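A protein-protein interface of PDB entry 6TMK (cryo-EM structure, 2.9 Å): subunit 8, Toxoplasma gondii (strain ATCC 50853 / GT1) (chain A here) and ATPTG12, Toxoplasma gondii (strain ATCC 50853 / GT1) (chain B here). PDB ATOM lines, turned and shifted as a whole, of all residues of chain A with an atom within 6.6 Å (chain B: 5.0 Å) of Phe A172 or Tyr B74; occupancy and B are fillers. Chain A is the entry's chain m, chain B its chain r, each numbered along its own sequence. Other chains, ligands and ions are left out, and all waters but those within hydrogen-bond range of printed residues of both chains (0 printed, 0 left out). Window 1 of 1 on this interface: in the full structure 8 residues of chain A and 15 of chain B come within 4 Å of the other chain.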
ATOM      1  N   PHE A 168      12.626  19.331  13.907  1.00  0.00           N
ATOM      2  CA  PHE A 168      13.988  18.826  13.900  1.00  0.00           C
ATOM      3  C   PHE A 168      14.145  17.431  14.473  1.00  0.00           C
ATOM      4  O   PHE A 168      15.082  16.734  14.083  1.00  0.00           O
ATOM      5  CB  PHE A 168      14.914  19.763  14.691  1.00  0.00           C
ATOM      6  CG  PHE A 168      15.062  21.137  14.103  1.00  0.00           C
ATOM      7  CD1 PHE A 168      14.634  21.421  12.825  1.00  0.00           C
ATOM      8  CD2 PHE A 168      15.645  22.145  14.841  1.00  0.00           C
ATOM      9  CE1 PHE A 168      14.782  22.681  12.297  1.00  0.00           C
ATOM     10  CE2 PHE A 168      15.795  23.403  14.318  1.00  0.00           C
ATOM     11  CZ  PHE A 168      15.364  23.672  13.045  1.00  0.00           C
ATOM     12  N   ALA A 169      13.275  16.998  15.384  1.00  0.00           N
ATOM     13  CA  ALA A 169      13.555  15.802  16.156  1.00  0.00           C
ATOM     14  C   ALA A 169      13.270  14.513  15.400  1.00  0.00           C
ATOM     15  O   ALA A 169      13.600  13.438  15.909  1.00  0.00           O
ATOM     16  CB  ALA A 169      12.738  15.830  17.447  1.00  0.00           C
ATOM     17  N   THR A 170      12.673  14.587  14.209  1.00  0.00           N
ATOM     18  CA  THR A 170      12.266  13.390  13.482  1.00  0.00           C
ATOM     19  C   THR A 170      12.619  13.480  12.003  1.00  0.00           C
ATOM     20  O   THR A 170      11.912  12.921  11.160  1.00  0.00           O
ATOM     21  CB  THR A 170      10.770  13.149  13.632  1.00  0.00           C
ATOM     22  OG1 THR A 170      10.068  14.374  13.401  1.00  0.00           O
ATOM     23  CG2 THR A 170      10.457  12.649  15.007  1.00  0.00           C
ATOM     24  N   ASN A 171      13.708  14.163  11.672  1.00  0.00           N
ATOM     25  CA  ASN A 171      14.075  14.416  10.287  1.00  0.00           C
ATOM     26  C   ASN A 171      14.995  13.339   9.721  1.00  0.00           C
ATOM     27  O   ASN A 171      14.791  12.877   8.595  1.00  0.00           O
ATOM     28  CB  ASN A 171      14.728  15.789  10.165  1.00  0.00           C
ATOM     29  CG  ASN A 171      14.650  16.343   8.766  1.00  0.00           C
ATOM     30  OD1 ASN A 171      14.892  15.636   7.790  1.00  0.00           O
ATOM     31  ND2 ASN A 171      14.301  17.611   8.658  1.00  0.00           N
ATOM     32  N   PHE A 172      16.011  12.945  10.490  1.00  0.00           N
ATOM     33  CA  PHE A 172      17.107  12.078  10.055  1.00  0.00           C
ATOM     34  C   PHE A 172      18.075  12.817   9.142  1.00  0.00           C
ATOM     35  O   PHE A 172      19.137  12.285   8.804  1.00  0.00           O
ATOM     36  CB  PHE A 172      16.601  10.830   9.323  1.00  0.00           C
ATOM     37  CG  PHE A 172      15.762   9.922  10.158  1.00  0.00           C
ATOM     38  CD1 PHE A 172      16.301   8.775  10.695  1.00  0.00           C
ATOM     39  CD2 PHE A 172      14.429  10.195  10.383  1.00  0.00           C
ATOM     40  CE1 PHE A 172      15.536   7.926  11.454  1.00  0.00           C
ATOM     41  CE2 PHE A 172      13.662   9.353  11.143  1.00  0.00           C
ATOM     42  CZ  PHE A 172      14.216   8.214  11.678  1.00  0.00           C
ATOM     43  N   LYS A 173      17.735  14.043   8.745  1.00  0.00           N
ATOM     44  CA  LYS A 173      18.610  14.858   7.922  1.00  0.00           C
ATOM     45  C   LYS A 173      19.273  15.985   8.690  1.00  0.00           C
ATOM     46  O   LYS A 173      20.270  16.532   8.212  1.00  0.00           O
ATOM     47  CB  LYS A 173      17.834  15.459   6.747  1.00  0.00           C
ATOM     48  CG  LYS A 173      17.092  14.438   5.922  1.00  0.00           C
ATOM     49  CD  LYS A 173      16.290  15.088   4.806  1.00  0.00           C
ATOM     50  CE  LYS A 173      17.166  15.903   3.868  1.00  0.00           C
ATOM     51  NZ  LYS A 173      18.443  15.223   3.519  1.00  0.00           N
ATOM     52  N   MET A 174      18.745  16.343   9.855  1.00  0.00           N
ATOM     53  CA  MET A 174      19.284  17.415  10.679  1.00  0.00           C
ATOM     54  C   MET A 174      19.894  16.768  11.915  1.00  0.00           C
ATOM     55  O   MET A 174      19.273  16.694  12.975  1.00  0.00           O
ATOM     56  CB  MET A 174      18.204  18.434  11.047  1.00  0.00           C
ATOM     57  CG  MET A 174      17.580  19.137   9.863  1.00  0.00           C
ATOM     58  SD  MET A 174      16.604  20.567  10.342  1.00  0.00           S
ATOM     59  CE  MET A 174      17.905  21.692  10.836  1.00  0.00           C
ATOM     60  N   VAL A 175      21.133  16.298  11.774  1.00  0.00           N
ATOM     61  CA  VAL A 175      21.892  15.928  12.959  1.00  0.00           C
ATOM     62  C   VAL A 175      22.355  17.183  13.673  1.00  0.00           C
ATOM     63  O   VAL A 175      22.471  17.205  14.904  1.00  0.00           O
ATOM     64  CB  VAL A 175      23.075  15.023  12.575  1.00  0.00           C
ATOM     65  CG1 VAL A 175      22.606  13.891  11.718  1.00  0.00           C
ATOM     66  CG2 VAL A 175      24.116  15.810  11.840  1.00  0.00           C
ATOM     67  N   ALA A 181      27.799  21.902   8.761  1.00  0.00           N
ATOM     68  CA  ALA A 181      28.011  20.566   8.231  1.00  0.00           C
ATOM     69  C   ALA A 181      29.437  20.346   7.749  1.00  0.00           C
ATOM     70  O   ALA A 181      29.825  19.198   7.515  1.00  0.00           O
ATOM     71  CB  ALA A 181      27.034  20.307   7.091  1.00  0.00           C
ATOM     72  N   LEU A 184      31.355  17.991  10.160  1.00  0.00           N
ATOM     73  CA  LEU A 184      31.005  16.594  10.305  1.00  0.00           C
ATOM     74  C   LEU A 184      32.076  15.703   9.685  1.00  0.00           C
ATOM     75  O   LEU A 184      32.834  16.137   8.816  1.00  0.00           O
ATOM     76  CB  LEU A 184      29.661  16.305   9.654  1.00  0.00           C
ATOM     77  CG  LEU A 184      28.419  16.698  10.441  1.00  0.00           C
ATOM     78  CD1 LEU A 184      27.183  16.397   9.643  1.00  0.00           C
ATOM     79  CD2 LEU A 184      28.384  15.960  11.760  1.00  0.00           C
ATOM     80  N   ASN A 187      31.219  10.799   4.664  1.00  0.00           N
ATOM     81  CA  ASN A 187      30.496   9.560   4.441  1.00  0.00           C
ATOM     82  C   ASN A 187      31.403   8.558   3.735  1.00  0.00           C
ATOM     83  O   ASN A 187      31.961   8.876   2.680  1.00  0.00           O
ATOM     84  CB  ASN A 187      29.251   9.812   3.610  1.00  0.00           C
ATOM     85  CG  ASN A 187      28.241   8.702   3.732  1.00  0.00           C
ATOM     86  OD1 ASN A 187      28.569   7.590   4.139  1.00  0.00           O
ATOM     87  ND2 ASN A 187      27.001   8.997   3.382  1.00  0.00           N
ATOM     88  N   MET B   1      15.210  10.674  15.133  1.00  0.00           N
ATOM     89  CA  MET B   1      14.863   9.913  16.365  1.00  0.00           C
ATOM     90  C   MET B   1      15.239  10.661  17.639  1.00  0.00           C
ATOM     91  O   MET B   1      16.046  11.587  17.616  1.00  0.00           O
ATOM     92  CB  MET B   1      15.547   8.548  16.350  1.00  0.00           C
ATOM     93  CG  MET B   1      17.035   8.591  16.578  1.00  0.00           C
ATOM     94  SD  MET B   1      17.916   7.390  15.572  1.00  0.00           S
ATOM     95  CE  MET B   1      17.918   8.211  13.984  1.00  0.00           C
ATOM     96  N   LYS B  70      23.019   8.525  15.159  1.00  0.00           N
ATOM     97  CA  LYS B  70      22.390   9.476  14.248  1.00  0.00           C
ATOM     98  C   LYS B  70      23.200   9.639  12.969  1.00  0.00           C
ATOM     99  O   LYS B  70      22.628   9.749  11.881  1.00  0.00           O
ATOM    100  CB  LYS B  70      22.209  10.822  14.942  1.00  0.00           C
ATOM    101  CG  LYS B  70      20.878  10.989  15.622  1.00  0.00           C
ATOM    102  CD  LYS B  70      20.711  12.390  16.159  1.00  0.00           C
ATOM    103  CE  LYS B  70      20.027  13.291  15.163  1.00  0.00           C
ATOM    104  NZ  LYS B  70      18.577  13.001  15.078  1.00  0.00           N
ATOM    105  N   LEU B  71      24.526   9.712  13.081  1.00  0.00           N
ATOM    106  CA  LEU B  71      25.354   9.906  11.897  1.00  0.00           C
ATOM    107  C   LEU B  71      25.283   8.704  10.975  1.00  0.00           C
ATOM    108  O   LEU B  71      25.275   8.857   9.752  1.00  0.00           O
ATOM    109  CB  LEU B  71      26.803  10.170  12.292  1.00  0.00           C
ATOM    110  CG  LEU B  71      27.141  11.538  12.854  1.00  0.00           C
ATOM    111  CD1 LEU B  71      28.534  11.537  13.409  1.00  0.00           C
ATOM    112  CD2 LEU B  71      27.050  12.527  11.723  1.00  0.00           C
ATOM    113  N   ASP B  72      25.247   7.501  11.539  1.00  0.00           N
ATOM    114  CA  ASP B  72      25.083   6.319  10.702  1.00  0.00           C
ATOM    115  C   ASP B  72      23.761   6.367   9.946  1.00  0.00           C
ATOM    116  O   ASP B  72      23.711   6.105   8.734  1.00  0.00           O
ATOM    117  CB  ASP B  72      25.172   5.062  11.558  1.00  0.00           C
ATOM    118  CG  ASP B  72      26.550   4.866  12.157  1.00  0.00           C
ATOM    119  OD1 ASP B  72      27.291   5.864  12.283  1.00  0.00           O
ATOM    120  OD2 ASP B  72      26.895   3.716  12.501  1.00  0.00           O
ATOM    121  N   ALA B  73      22.683   6.730  10.642  1.00  0.00           N
ATOM    122  CA  ALA B  73      21.394   6.895   9.976  1.00  0.00           C
ATOM    123  C   ALA B  73      21.467   7.936   8.865  1.00  0.00           C
ATOM    124  O   ALA B  73      20.978   7.711   7.751  1.00  0.00           O
ATOM    125  CB  ALA B  73      20.327   7.279  10.995  1.00  0.00           C
ATOM    126  N   TYR B  74      22.060   9.093   9.156  1.00  0.00           N
ATOM    127  CA  TYR B  74      22.130  10.171   8.176  1.00  0.00           C
ATOM    128  C   TYR B  74      22.949   9.762   6.963  1.00  0.00           C
ATOM    129  O   TYR B  74      22.604  10.104   5.826  1.00  0.00           O
ATOM    130  CB  TYR B  74      22.721  11.418   8.832  1.00  0.00           C
ATOM    131  CG  TYR B  74      23.038  12.538   7.876  1.00  0.00           C
ATOM    132  CD1 TYR B  74      22.060  13.079   7.060  1.00  0.00           C
ATOM    133  CD2 TYR B  74      24.316  13.063   7.801  1.00  0.00           C
ATOM    134  CE1 TYR B  74      22.348  14.102   6.190  1.00  0.00           C
ATOM    135  CE2 TYR B  74      24.614  14.087   6.936  1.00  0.00           C
ATOM    136  CZ  TYR B  74      23.627  14.605   6.132  1.00  0.00           C
ATOM    137  OH  TYR B  74      23.920  15.631   5.264  1.00  0.00           O
ATOM    138  N   HIS B  75      24.049   9.046   7.185  1.00  0.00           N
ATOM    139  CA  HIS B  75      24.871   8.589   6.076  1.00  0.00           C
ATOM    140  C   HIS B  75      24.093   7.635   5.186  1.00  0.00           C
ATOM    141  O   HIS B  75      24.107   7.764   3.957  1.00  0.00           O
ATOM    142  CB  HIS B  75      26.139   7.932   6.606  1.00  0.00           C
ATOM    143  CG  HIS B  75      27.122   8.900   7.184  1.00  0.00           C
ATOM    144  ND1 HIS B  75      27.134  10.235   6.847  1.00  0.00           N
ATOM    145  CD2 HIS B  75      28.133   8.725   8.066  1.00  0.00           C
ATOM    146  CE1 HIS B  75      28.108  10.842   7.499  1.00  0.00           C
ATOM    147  NE2 HIS B  75      28.728   9.948   8.246  1.00  0.00           N
ATOM    148  N   LEU B  76      23.403   6.666   5.791  1.00  0.00           N
ATOM    149  CA  LEU B  76      22.587   5.760   4.988  1.00  0.00           C
ATOM    150  C   LEU B  76      21.525   6.523   4.207  1.00  0.00           C
ATOM    151  O   LEU B  76      21.272   6.226   3.033  1.00  0.00           O
ATOM    152  CB  LEU B  76      21.941   4.706   5.879  1.00  0.00           C
ATOM    153  CG  LEU B  76      22.896   3.710   6.526  1.00  0.00           C
ATOM    154  CD1 LEU B  76      22.174   2.882   7.543  1.00  0.00           C
ATOM    155  CD2 LEU B  76      23.516   2.819   5.480  1.00  0.00           C
ATOM    156  N   LEU B  77      20.912   7.527   4.830  1.00  0.00           N
ATOM    157  CA  LEU B  77      19.850   8.271   4.162  1.00  0.00           C
ATOM    158  C   LEU B  77      20.384   9.057   2.972  1.00  0.00           C
ATOM    159  O   LEU B  77      19.797   9.036   1.883  1.00  0.00           O
ATOM    160  CB  LEU B  77      19.166   9.199   5.160  1.00  0.00           C
ATOM    161  CG  LEU B  77      18.031  10.048   4.600  1.00  0.00           C
ATOM    162  CD1 LEU B  77      16.894  10.082   5.575  1.00  0.00           C
ATOM    163  CD2 LEU B  77      18.512  11.452   4.314  1.00  0.00           C
ATOM    164  N   GLU B  78      21.492   9.775   3.160  1.00  0.00           N
ATOM    165  CA  GLU B  78      22.024  10.560   2.054  1.00  0.00           C
ATOM    166  C   GLU B  78      22.584   9.664   0.959  1.00  0.00           C
ATOM    167  O   GLU B  78      22.533  10.028  -0.220  1.00  0.00           O
ATOM    168  CB  GLU B  78      23.091  11.529   2.555  1.00  0.00           C
ATOM    169  CG  GLU B  78      24.329  10.873   3.100  1.00  0.00           C
ATOM    170  CD  GLU B  78      25.368  11.882   3.546  1.00  0.00           C
ATOM    171  OE1 GLU B  78      25.059  13.091   3.549  1.00  0.00           O
ATOM    172  OE2 GLU B  78      26.495  11.467   3.889  1.00  0.00           O
ATOM    173  N   ALA B  79      23.098   8.486   1.317  1.00  0.00           N
ATOM    174  CA  ALA B  79      23.484   7.521   0.296  1.00  0.00           C
ATOM    175  C   ALA B  79      22.273   7.062  -0.504  1.00  0.00           C
ATOM    176  O   ALA B  79      22.348   6.910  -1.728  1.00  0.00           O
ATOM    177  CB  ALA B  79      24.179   6.328   0.942  1.00  0.00           C
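O of His B75 sits at hydrogen-bond distance from ND2 of Asn A187, 3.2 Å away.
ND2 of Asn A187 sits at hydrogen-bond distance from OE2 of Glu B78 (2.6 Å).
O of Ala A169 is in hydrogen-bond range of N of Met B1.
The side-chain hydroxyl (OH) of Tyr B74 is in hydrogen-bond range of the side-chain carboxylate (OE1) of Glu B78 (3.3 Å).
The side-chain amide oxygen of Asn A171 sits close to the backbone NH of Lys A173, 3.4 Å away.
The side-chain carboxylate (OE2) of Glu B78 lies within hydrogen-bond range of a ring nitrogen (ND1) of His B75, at 3.3 Å.
Among the printed residues, merely in contact across the chains: Phe A172 with Met B1, Phe A172 with Tyr B74, Lys A173 with Leu B77, Leu A184 with Leu B71, Lys A173 with Tyr B74, Val A175 with Tyr B74, Phe A172 with Leu B77 and Val A175 with Lys B70.
Printed residues of chain B within 4 Å of Ala A169: Met B1 (3.3 Å).
Asn A171 touches none of the printed residues of chain B.
Phe A172 touches just these residues of chain B: Met B1, Tyr B74 and Leu B77.
Met A174 touches none of the printed residues of chain B.
Of the printed residues of chain B, Leu A184 touches Leu B71 (3.7 Å).
Of the printed residues of chain B, Asn A187 touches His B75 (3.2 Å) and Glu B78 (2.6 Å).
Printed residues of chain A within 4 Å of Met B1: Ala A169 and Phe A172.
The nearest residue of chain B that does not touch Phe A172 is Ala B73 (4.3 Å).
The nearest residue of chain A that does not touch Tyr B74 is Leu A184 (4.4 Å).
Of the 11 printed residues of chain B, 7 touch a printed residue of chain A.
Printed residues of chain B that touch a printed residue of chain A: Met B1, Lys B70, Leu B71, Tyr B74, His B75, Leu B77 and Glu B78.
Along chain B the printed residues that touch a printed residue of chain A span positions 1 to 78.
Hydrophobic or aromatic side chains of chain A within 4 Å of the printed part of chain B: Phe A172, Val A175 and Leu A184.
Among the printed residues, 11 pairs touch across the chains.
Among the printed residues, no Asp or Glu carboxylate lies within 4 Å of a Lys or Arg side-chain nitrogen of the other chain.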
